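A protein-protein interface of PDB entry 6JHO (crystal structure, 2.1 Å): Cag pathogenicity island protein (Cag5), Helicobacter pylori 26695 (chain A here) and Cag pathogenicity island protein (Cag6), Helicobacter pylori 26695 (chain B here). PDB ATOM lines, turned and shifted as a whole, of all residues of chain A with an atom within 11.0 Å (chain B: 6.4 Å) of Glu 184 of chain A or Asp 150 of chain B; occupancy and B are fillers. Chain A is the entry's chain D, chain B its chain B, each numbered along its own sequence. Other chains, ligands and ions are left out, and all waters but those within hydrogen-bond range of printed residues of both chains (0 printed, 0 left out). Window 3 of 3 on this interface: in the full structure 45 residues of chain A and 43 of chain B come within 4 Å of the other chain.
The side-chain carboxylate (OD1) of Asp 150 of chain B sits at hydrogen-bond distance from the backbone NH (N) of Asn 152 of chain B, at 3.3 Å.
The side-chain carboxylate of Asp 150 of chain B lies within hydrogen-bond range of the backbone NH of Met 153 of chain B (2.9 Å).
O of Met 179 of chain A sits at hydrogen-bond distance from OG1 of Thr 185 of chain A.
The backbone carbonyl oxygen (O) of Gly 180 of chain A is in hydrogen-bond range of the side-chain hydroxyl (OG1) of Thr 185 of chain A (2.8 Å).
O of Ala 182 of chain A lies within hydrogen-bond range of OG1 of Thr 185 of chain A (3.4 Å).
Of the 12 printed residues of chain B, 6 touch a printed residue of chain A.
Printed residues of chain B that touch a printed residue of chain A: Arg 142, Asp 150, Gly 151, Asn 152, Met 154 and Gly 155.
Hydrophobic or aromatic side chains of chain B within 4 Å of the printed part of chain A: Met 154.
Along chain B the printed residues that touch a printed residue of chain A span positions 142 to 155.
Of the 21 printed residues of chain A, 4 touch a printed residue of chain B.
Along chain A the printed residues that touch a printed residue of chain B span positions 80 to 185.
Among the printed residues, merely in contact across the chains: Glu 184 of chain A with Gly 151 of chain B (3.1 Å), Phe 81 of chain A with Gly 151 of chain B (3.4 Å), Phe 81 of chain A with Asn 152 of chain B (3.5 Å), Glu 184 of chain A with Met 154 of chain B (3.5 Å), Thr 185 of chain A with Gly 151 of chain B (3.5 Å), Thr 185 of chain A with Met 154 of chain B (3.6 Å), Phe 80 of chain A with Gly 155 of chain B (3.7 Å) and Glu 184 of chain A with Asp 150 of chain B (3.96 Å).
NH2 of Arg 142 of chain B is in salt-bridge range of OE2 of Glu 184 of chain A (2.4 Å).
Of the printed residues of chain B, Phe 80 of chain A touches Gly 155.
Printed residues of chain B within 4 Å of Phe 81 of chain A: Gly 151 and Asn 152.
Gly 180 of chain A touches none of the printed residues of chain B.
Of chain B, only Arg 142 (2.4 Å), Asp 150 (3.96 Å), Gly 151 (3.1 Å) and Met 154 (3.5 Å) come within 4 Å of Glu 184 of chain A.
Printed residues of chain B within 4 Å of Thr 185 of chain A: Gly 151 and Met 154.
Ser 187 of chain A touches none of the printed residues of chain B.
Of the printed residues of chain A, Arg 142 of chain B touches Glu 184.
Asp 150 of chain B touches just one residue of chain A: Glu 184 (3.96 Å).
Asn 152 of chain B touches just one residue of chain A: Phe 81 (3.5 Å).
No residue of chain A comes within 4 Å of Met 153 of chain B.
Met 154 of chain B touches two residues of chain A.
Printed residues of chain A within 4 Å of Gly 155 of chain B: Phe 80.
The nearest printed residue of chain B that does not touch Phe 80 of chain A is Met 154 of chain B (5.3 Å).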
ATOM      1  N   ASP A  78      25.922  24.299   3.907  1.00  0.00           N
ATOM      2  CA  ASP A  78      24.916  24.456   4.957  1.00  0.00           C
ATOM      3  C   ASP A  78      23.864  25.502   4.583  1.00  0.00           C
ATOM      4  O   ASP A  78      23.868  26.617   5.127  1.00  0.00           O
ATOM      5  CB  ASP A  78      25.585  24.816   6.295  1.00  0.00           C
ATOM      6  CG  ASP A  78      26.676  23.829   6.693  1.00  0.00           C
ATOM      7  OD1 ASP A  78      26.405  22.600   6.671  1.00  0.00           O
ATOM      8  OD2 ASP A  78      27.803  24.273   7.024  1.00  0.00           O
ATOM      9  N   PHE A  80      20.783  25.223   5.412  1.00  0.00           N
ATOM     10  CA  PHE A  80      19.899  25.297   6.574  1.00  0.00           C
ATOM     11  C   PHE A  80      20.317  26.424   7.510  1.00  0.00           C
ATOM     12  O   PHE A  80      19.481  27.237   7.917  1.00  0.00           O
ATOM     13  CB  PHE A  80      19.874  23.956   7.321  1.00  0.00           C
ATOM     14  CG  PHE A  80      19.081  23.977   8.627  1.00  0.00           C
ATOM     15  CD1 PHE A  80      17.684  23.974   8.621  1.00  0.00           C
ATOM     16  CD2 PHE A  80      19.738  23.968   9.855  1.00  0.00           C
ATOM     17  CE1 PHE A  80      16.962  23.963   9.806  1.00  0.00           C
ATOM     18  CE2 PHE A  80      19.017  23.968  11.062  1.00  0.00           C
ATOM     19  CZ  PHE A  80      17.625  23.961  11.035  1.00  0.00           C
ATOM     20  N   PHE A  81      21.607  26.494   7.860  1.00  0.00           N
ATOM     21  CA  PHE A  81      22.063  27.529   8.794  1.00  0.00           C
ATOM     22  C   PHE A  81      21.803  28.921   8.238  1.00  0.00           C
ATOM     23  O   PHE A  81      21.371  29.829   8.963  1.00  0.00           O
ATOM     24  CB  PHE A  81      23.562  27.367   9.090  1.00  0.00           C
ATOM     25  CG  PHE A  81      23.921  26.107   9.859  1.00  0.00           C
ATOM     26  CD1 PHE A  81      23.031  25.530  10.746  1.00  0.00           C
ATOM     27  CD2 PHE A  81      25.167  25.515   9.694  1.00  0.00           C
ATOM     28  CE1 PHE A  81      23.365  24.374  11.449  1.00  0.00           C
ATOM     29  CE2 PHE A  81      25.514  24.365  10.402  1.00  0.00           C
ATOM     30  CZ  PHE A  81      24.603  23.794  11.271  1.00  0.00           C
ATOM     31  N   GLN A  84      18.079  29.710   8.254  1.00  0.00           N
ATOM     32  CA  GLN A  84      17.590  29.990   9.589  1.00  0.00           C
ATOM     33  C   GLN A  84      18.145  31.303  10.122  1.00  0.00           C
ATOM     34  O   GLN A  84      17.481  31.976  10.920  1.00  0.00           O
ATOM     35  CB  GLN A  84      17.932  28.822  10.511  1.00  0.00           C
ATOM     36  CG  GLN A  84      17.175  27.548  10.151  1.00  0.00           C
ATOM     37  CD  GLN A  84      15.681  27.675  10.432  1.00  0.00           C
ATOM     38  OE1 GLN A  84      15.273  28.114  11.514  1.00  0.00           O
ATOM     39  NE2 GLN A  84      14.861  27.301   9.454  1.00  0.00           N
ATOM     40  N   MET A 148      16.077  33.406  23.823  1.00  0.00           N
ATOM     41  CA  MET A 148      15.509  32.154  24.316  1.00  0.00           C
ATOM     42  C   MET A 148      15.028  32.285  25.757  1.00  0.00           C
ATOM     43  O   MET A 148      13.954  31.786  26.114  1.00  0.00           O
ATOM     44  CB  MET A 148      16.547  31.037  24.205  1.00  0.00           C
ATOM     45  CG  MET A 148      16.697  30.440  22.805  1.00  0.00           C
ATOM     46  SD  MET A 148      15.385  29.283  22.322  1.00  0.00           S
ATOM     47  CE  MET A 148      14.666  28.757  23.889  1.00  0.00           C
ATOM     48  N   PHE A 176      11.212  29.008  14.733  1.00  0.00           N
ATOM     49  CA  PHE A 176      12.664  29.057  14.850  1.00  0.00           C
ATOM     50  C   PHE A 176      13.164  28.176  16.001  1.00  0.00           C
ATOM     51  O   PHE A 176      14.132  27.425  15.830  1.00  0.00           O
ATOM     52  CB  PHE A 176      13.122  30.513  15.002  1.00  0.00           C
ATOM     53  CG  PHE A 176      14.617  30.673  15.108  1.00  0.00           C
ATOM     54  CD1 PHE A 176      15.405  30.806  13.965  1.00  0.00           C
ATOM     55  CD2 PHE A 176      15.236  30.673  16.352  1.00  0.00           C
ATOM     56  CE1 PHE A 176      16.795  30.943  14.064  1.00  0.00           C
ATOM     57  CE2 PHE A 176      16.629  30.817  16.470  1.00  0.00           C
ATOM     58  CZ  PHE A 176      17.403  30.952  15.324  1.00  0.00           C
ATOM     59  N   LYS A 177      12.494  28.203  17.160  1.00  0.00           N
ATOM     60  CA  LYS A 177      12.951  27.379  18.283  1.00  0.00           C
ATOM     61  C   LYS A 177      12.900  25.899  17.940  1.00  0.00           C
ATOM     62  O   LYS A 177      13.661  25.091  18.487  1.00  0.00           O
ATOM     63  CB  LYS A 177      12.105  27.659  19.521  1.00  0.00           C
ATOM     64  CG  LYS A 177      12.535  28.897  20.279  1.00  0.00           C
ATOM     65  CD  LYS A 177      11.341  29.596  20.935  1.00  0.00           C
ATOM     66  CE  LYS A 177      10.858  28.870  22.163  1.00  0.00           C
ATOM     67  NZ  LYS A 177       9.790  29.672  22.847  1.00  0.00           N
ATOM     68  N   THR A 178      12.042  25.549  17.011  1.00  0.00           N
ATOM     69  CA  THR A 178      11.840  24.196  16.554  1.00  0.00           C
ATOM     70  C   THR A 178      12.839  23.780  15.462  1.00  0.00           C
ATOM     71  O   THR A 178      13.064  22.576  15.253  1.00  0.00           O
ATOM     72  CB  THR A 178      10.370  24.154  16.111  1.00  0.00           C
ATOM     73  OG1 THR A 178       9.490  23.972  17.233  1.00  0.00           O
ATOM     74  CG2 THR A 178      10.133  23.226  15.081  1.00  0.00           C
ATOM     75  N   MET A 179      13.476  24.748  14.792  1.00  0.00           N
ATOM     76  CA  MET A 179      14.355  24.470  13.668  1.00  0.00           C
ATOM     77  C   MET A 179      15.746  25.017  13.989  1.00  0.00           C
ATOM     78  O   MET A 179      16.499  24.380  14.731  1.00  0.00           O
ATOM     79  CB  MET A 179      13.806  25.073  12.373  1.00  0.00           C
ATOM     80  CG  MET A 179      12.338  24.849  12.171  1.00  0.00           C
ATOM     81  SD  MET A 179      12.043  23.680  10.868  1.00  0.00           S
ATOM     82  CE  MET A 179      11.929  24.719   9.455  1.00  0.00           C
ATOM     83  N   GLY A 180      16.125  26.174  13.426  1.00  0.00           N
ATOM     84  CA  GLY A 180      17.461  26.712  13.649  1.00  0.00           C
ATOM     85  C   GLY A 180      17.787  26.973  15.107  1.00  0.00           C
ATOM     86  O   GLY A 180      18.952  26.885  15.515  1.00  0.00           O
ATOM     87  N   GLY A 181      16.778  27.299  15.911  1.00  0.00           N
ATOM     88  CA  GLY A 181      16.992  27.485  17.327  1.00  0.00           C
ATOM     89  C   GLY A 181      17.105  26.213  18.126  1.00  0.00           C
ATOM     90  O   GLY A 181      17.174  26.266  19.355  1.00  0.00           O
ATOM     91  N   ALA A 182      17.121  25.056  17.476  1.00  0.00           N
ATOM     92  CA  ALA A 182      17.269  23.812  18.221  1.00  0.00           C
ATOM     93  C   ALA A 182      18.579  23.821  19.003  1.00  0.00           C
ATOM     94  O   ALA A 182      19.527  24.529  18.654  1.00  0.00           O
ATOM     95  CB  ALA A 182      17.219  22.599  17.280  1.00  0.00           C
ATOM     96  N   ARG A 183      18.607  23.034  20.083  1.00  0.00           N
ATOM     97  CA  ARG A 183      19.763  23.007  20.978  1.00  0.00           C
ATOM     98  C   ARG A 183      21.064  22.781  20.213  1.00  0.00           C
ATOM     99  O   ARG A 183      22.069  23.463  20.448  1.00  0.00           O
ATOM    100  CB  ARG A 183      19.562  21.917  22.029  1.00  0.00           C
ATOM    101  CG  ARG A 183      20.622  21.873  23.105  1.00  0.00           C
ATOM    102  CD  ARG A 183      20.911  20.431  23.509  1.00  0.00           C
ATOM    103  NE  ARG A 183      20.118  20.006  24.662  1.00  0.00           N
ATOM    104  CZ  ARG A 183      20.459  20.243  25.928  1.00  0.00           C
ATOM    105  NH1 ARG A 183      21.580  20.907  26.199  1.00  0.00           N
ATOM    106  NH2 ARG A 183      19.683  19.819  26.920  1.00  0.00           N
ATOM    107  N   GLU A 184      21.054  21.837  19.271  1.00  0.00           N
ATOM    108  CA  GLU A 184      22.275  21.459  18.572  1.00  0.00           C
ATOM    109  C   GLU A 184      22.696  22.487  17.532  1.00  0.00           C
ATOM    110  O   GLU A 184      23.894  22.628  17.268  1.00  0.00           O
ATOM    111  CB  GLU A 184      22.094  20.096  17.896  1.00  0.00           C
ATOM    112  CG  GLU A 184      21.818  18.943  18.843  1.00  0.00           C
ATOM    113  CD  GLU A 184      20.403  18.946  19.388  1.00  0.00           C
ATOM    114  OE1 GLU A 184      19.550  19.678  18.841  1.00  0.00           O
ATOM    115  OE2 GLU A 184      20.143  18.219  20.369  1.00  0.00           O
ATOM    116  N   THR A 185      21.748  23.189  16.908  1.00  0.00           N
ATOM    117  CA  THR A 185      22.073  24.051  15.775  1.00  0.00           C
ATOM    118  C   THR A 185      22.221  25.526  16.133  1.00  0.00           C
ATOM    119  O   THR A 185      22.755  26.290  15.316  1.00  0.00           O
ATOM    120  CB  THR A 185      20.995  23.935  14.687  1.00  0.00           C
ATOM    121  OG1 THR A 185      19.706  24.162  15.277  1.00  0.00           O
ATOM    122  CG2 THR A 185      21.039  22.544  14.015  1.00  0.00           C
ATOM    123  N   TYR A 186      21.748  25.947  17.306  1.00  0.00           N
ATOM    124  CA  TYR A 186      21.576  27.373  17.585  1.00  0.00           C
ATOM    125  C   TYR A 186      22.866  28.165  17.390  1.00  0.00           C
ATOM    126  O   TYR A 186      22.887  29.176  16.673  1.00  0.00           O
ATOM    127  CB  TYR A 186      21.063  27.573  19.005  1.00  0.00           C
ATOM    128  CG  TYR A 186      20.541  28.969  19.240  1.00  0.00           C
ATOM    129  CD1 TYR A 186      20.080  29.744  18.179  1.00  0.00           C
ATOM    130  CD2 TYR A 186      20.514  29.520  20.513  1.00  0.00           C
ATOM    131  CE1 TYR A 186      19.598  31.020  18.374  1.00  0.00           C
ATOM    132  CE2 TYR A 186      20.029  30.801  20.720  1.00  0.00           C
ATOM    133  CZ  TYR A 186      19.565  31.543  19.642  1.00  0.00           C
ATOM    134  OH  TYR A 186      19.077  32.819  19.833  1.00  0.00           O
ATOM    135  N   SER A 187      23.949  27.750  18.060  1.00  0.00           N
ATOM    136  CA  SER A 187      25.176  28.548  17.986  1.00  0.00           C
ATOM    137  C   SER A 187      25.715  28.613  16.562  1.00  0.00           C
ATOM    138  O   SER A 187      26.267  29.639  16.153  1.00  0.00           O
ATOM    139  CB  SER A 187      26.224  27.992  18.946  1.00  0.00           C
ATOM    140  OG  SER A 187      26.879  26.883  18.371  1.00  0.00           O
ATOM    141  N   SER A 188      25.536  27.553  15.770  1.00  0.00           N
ATOM    142  CA  SER A 188      25.982  27.628  14.384  1.00  0.00           C
ATOM    143  C   SER A 188      25.117  28.590  13.578  1.00  0.00           C
ATOM    144  O   SER A 188      25.619  29.262  12.663  1.00  0.00           O
ATOM    145  CB  SER A 188      25.980  26.236  13.753  1.00  0.00           C
ATOM    146  OG  SER A 188      26.364  25.256  14.712  1.00  0.00           O
ATOM    147  N   VAL A 189      23.823  28.690  13.905  1.00  0.00           N
ATOM    148  CA  VAL A 189      22.990  29.682  13.232  1.00  0.00           C
ATOM    149  C   VAL A 189      23.432  31.087  13.621  1.00  0.00           C
ATOM    150  O   VAL A 189      23.584  31.963  12.763  1.00  0.00           O
ATOM    151  CB  VAL A 189      21.496  29.439  13.533  1.00  0.00           C
ATOM    152  CG1 VAL A 189      20.639  30.583  12.965  1.00  0.00           C
ATOM    153  CG2 VAL A 189      21.056  28.093  12.933  1.00  0.00           C
ATOM    154  N   GLN A 190      23.671  31.311  14.922  1.00  0.00           N
ATOM    155  CA  GLN A 190      24.158  32.611  15.394  1.00  0.00           C
ATOM    156  C   GLN A 190      25.501  32.961  14.770  1.00  0.00           C
ATOM    157  O   GLN A 190      25.761  34.129  14.450  1.00  0.00           O
ATOM    158  CB  GLN A 190      24.299  32.616  16.913  1.00  0.00           C
ATOM    159  CG  GLN A 190      23.018  32.534  17.683  1.00  0.00           C
ATOM    160  CD  GLN A 190      23.243  32.760  19.169  1.00  0.00           C
ATOM    161  OE1 GLN A 190      23.553  31.825  19.913  1.00  0.00           O
ATOM    162  NE2 GLN A 190      23.095  34.007  19.610  1.00  0.00           N
ATOM    163  N   GLY A 191      26.371  31.964  14.601  1.00  0.00           N
ATOM    164  CA  GLY A 191      27.619  32.197  13.883  1.00  0.00           C
ATOM    165  C   GLY A 191      27.394  32.665  12.457  1.00  0.00           C
ATOM    166  O   GLY A 191      27.982  33.654  12.017  1.00  0.00           O
ATOM    167  N   PRO B  54      28.322   9.558  12.690  1.00  0.00           N
ATOM    168  CA  PRO B  54      27.589  10.599  11.945  1.00  0.00           C
ATOM    169  C   PRO B  54      27.213  10.200  10.529  1.00  0.00           C
ATOM    170  O   PRO B  54      26.088  10.472  10.083  1.00  0.00           O
ATOM    171  CB  PRO B  54      28.572  11.781  11.959  1.00  0.00           C
ATOM    172  CG  PRO B  54      29.273  11.633  13.261  1.00  0.00           C
ATOM    173  CD  PRO B  54      29.446  10.138  13.451  1.00  0.00           C
ATOM    174  N   ARG B 142      12.978  14.220  18.089  1.00  0.00           N
ATOM    175  CA  ARG B 142      13.947  14.425  19.157  1.00  0.00           C
ATOM    176  C   ARG B 142      14.185  13.148  19.961  1.00  0.00           C
ATOM    177  O   ARG B 142      15.336  12.792  20.239  1.00  0.00           O
ATOM    178  CB  ARG B 142      13.510  15.582  20.048  1.00  0.00           C
ATOM    179  CG  ARG B 142      13.685  16.945  19.379  1.00  0.00           C
ATOM    180  CD  ARG B 142      14.157  18.043  20.356  1.00  0.00           C
ATOM    181  NE  ARG B 142      15.494  17.788  20.914  1.00  0.00           N
ATOM    182  CZ  ARG B 142      16.634  18.259  20.404  1.00  0.00           C
ATOM    183  NH1 ARG B 142      16.618  19.007  19.307  1.00  0.00           N
ATOM    184  NH2 ARG B 142      17.793  17.973  20.988  1.00  0.00           N
ATOM    185  N   LEU B 145      17.211  10.915  18.430  1.00  0.00           N
ATOM    186  CA  LEU B 145      18.547  11.288  17.960  1.00  0.00           C
ATOM    187  C   LEU B 145      19.615  10.468  18.681  1.00  0.00           C
ATOM    188  O   LEU B 145      19.519  10.249  19.894  1.00  0.00           O
ATOM    189  CB  LEU B 145      18.871  12.770  18.171  1.00  0.00           C
ATOM    190  CG  LEU B 145      18.190  13.922  17.447  1.00  0.00           C
ATOM    191  CD1 LEU B 145      18.201  13.720  15.921  1.00  0.00           C
ATOM    192  CD2 LEU B 145      16.852  14.154  18.007  1.00  0.00           C
ATOM    193  N   PRO B 146      20.664  10.059  17.979  1.00  0.00           N
ATOM    194  CA  PRO B 146      21.781   9.362  18.623  1.00  0.00           C
ATOM    195  C   PRO B 146      22.497  10.278  19.602  1.00  0.00           C
ATOM    196  O   PRO B 146      22.410  11.513  19.489  1.00  0.00           O
ATOM    197  CB  PRO B 146      22.680   8.983  17.435  1.00  0.00           C
ATOM    198  CG  PRO B 146      22.379  10.016  16.394  1.00  0.00           C
ATOM    199  CD  PRO B 146      20.917  10.334  16.557  1.00  0.00           C
ATOM    200  N   PHE B 148      25.542  11.260  20.109  1.00  0.00           N
ATOM    201  CA  PHE B 148      26.591  12.123  19.579  1.00  0.00           C
ATOM    202  C   PHE B 148      26.082  13.167  18.592  1.00  0.00           C
ATOM    203  O   PHE B 148      26.892  13.722  17.835  1.00  0.00           O
ATOM    204  CB  PHE B 148      27.662  11.281  18.886  1.00  0.00           C
ATOM    205  CG  PHE B 148      27.108  10.275  17.903  1.00  0.00           C
ATOM    206  CD1 PHE B 148      26.882  10.624  16.578  1.00  0.00           C
ATOM    207  CD2 PHE B 148      26.829   8.975  18.305  1.00  0.00           C
ATOM    208  CE1 PHE B 148      26.379   9.703  15.684  1.00  0.00           C
ATOM    209  CE2 PHE B 148      26.330   8.044  17.410  1.00  0.00           C
ATOM    210  CZ  PHE B 148      26.105   8.410  16.096  1.00  0.00           C
ATOM    211  N   ILE B 149      24.769  13.426  18.559  1.00  0.00           N
ATOM    212  CA  ILE B 149      24.207  14.347  17.567  1.00  0.00           C
ATOM    213  C   ILE B 149      24.829  15.725  17.749  1.00  0.00           C
ATOM    214  O   ILE B 149      24.927  16.232  18.872  1.00  0.00           O
ATOM    215  CB  ILE B 149      22.670  14.376  17.685  1.00  0.00           C
ATOM    216  CG1 ILE B 149      22.032  15.204  16.563  1.00  0.00           C
ATOM    217  CG2 ILE B 149      22.224  14.889  19.049  1.00  0.00           C
ATOM    218  CD1 ILE B 149      22.025  14.511  15.206  1.00  0.00           C
ATOM    219  N   ASP B 150      25.301  16.321  16.658  1.00  0.00           N
ATOM    220  CA  ASP B 150      25.826  17.680  16.712  1.00  0.00           C
ATOM    221  C   ASP B 150      25.049  18.582  15.742  1.00  0.00           C
ATOM    222  O   ASP B 150      24.105  18.150  15.066  1.00  0.00           O
ATOM    223  CB  ASP B 150      27.340  17.693  16.448  1.00  0.00           C
ATOM    224  CG  ASP B 150      27.699  17.404  15.011  1.00  0.00           C
ATOM    225  OD1 ASP B 150      26.803  17.143  14.185  1.00  0.00           O
ATOM    226  OD2 ASP B 150      28.908  17.413  14.701  1.00  0.00           O
ATOM    227  N   GLY B 151      25.463  19.845  15.674  1.00  0.00           N
ATOM    228  CA  GLY B 151      24.722  20.815  14.887  1.00  0.00           C
ATOM    229  C   GLY B 151      24.784  20.548  13.394  1.00  0.00           C
ATOM    230  O   GLY B 151      23.820  20.801  12.668  1.00  0.00           O
ATOM    231  N   ASN B 152      25.913  20.030  12.913  1.00  0.00           N
ATOM    232  CA  ASN B 152      26.046  19.801  11.479  1.00  0.00           C
ATOM    233  C   ASN B 152      25.251  18.586  11.027  1.00  0.00           C
ATOM    234  O   ASN B 152      24.628  18.616   9.964  1.00  0.00           O
ATOM    235  CB  ASN B 152      27.515  19.665  11.112  1.00  0.00           C
ATOM    236  CG  ASN B 152      28.308  20.872  11.538  1.00  0.00           C
ATOM    237  OD1 ASN B 152      27.916  22.011  11.262  1.00  0.00           O
ATOM    238  ND2 ASN B 152      29.406  20.643  12.238  1.00  0.00           N
ATOM    239  N   MET B 153      25.267  17.508  11.809  1.00  0.00           N
ATOM    240  CA  MET B 153      24.409  16.368  11.504  1.00  0.00           C
ATOM    241  C   MET B 153      22.944  16.784  11.496  1.00  0.00           C
ATOM    242  O   MET B 153      22.162  16.350  10.640  1.00  0.00           O
ATOM    243  CB  MET B 153      24.612  15.256  12.532  1.00  0.00           C
ATOM    244  CG  MET B 153      25.977  14.576  12.537  1.00  0.00           C
ATOM    245  SD  MET B 153      26.158  13.723  14.118  1.00  0.00           S
ATOM    246  CE  MET B 153      24.852  12.516  14.068  1.00  0.00           C
ATOM    247  N   MET B 154      22.555  17.591  12.477  1.00  0.00           N
ATOM    248  CA  MET B 154      21.188  18.080  12.576  1.00  0.00           C
ATOM    249  C   MET B 154      20.814  18.903  11.350  1.00  0.00           C
ATOM    250  O   MET B 154      19.750  18.701  10.749  1.00  0.00           O
ATOM    251  CB  MET B 154      21.048  18.902  13.849  1.00  0.00           C
ATOM    252  CG  MET B 154      19.653  19.008  14.347  1.00  0.00           C
ATOM    253  SD  MET B 154      19.258  17.627  15.427  1.00  0.00           S
ATOM    254  CE  MET B 154      17.749  18.273  16.157  1.00  0.00           C
ATOM    255  N   GLY B 155      21.690  19.830  10.956  1.00  0.00           N
ATOM    256  CA  GLY B 155      21.408  20.664   9.801  1.00  0.00           C
ATOM    257  C   GLY B 155      21.254  19.855   8.531  1.00  0.00           C
ATOM    258  O   GLY B 155      20.305  20.052   7.770  1.00  0.00           O
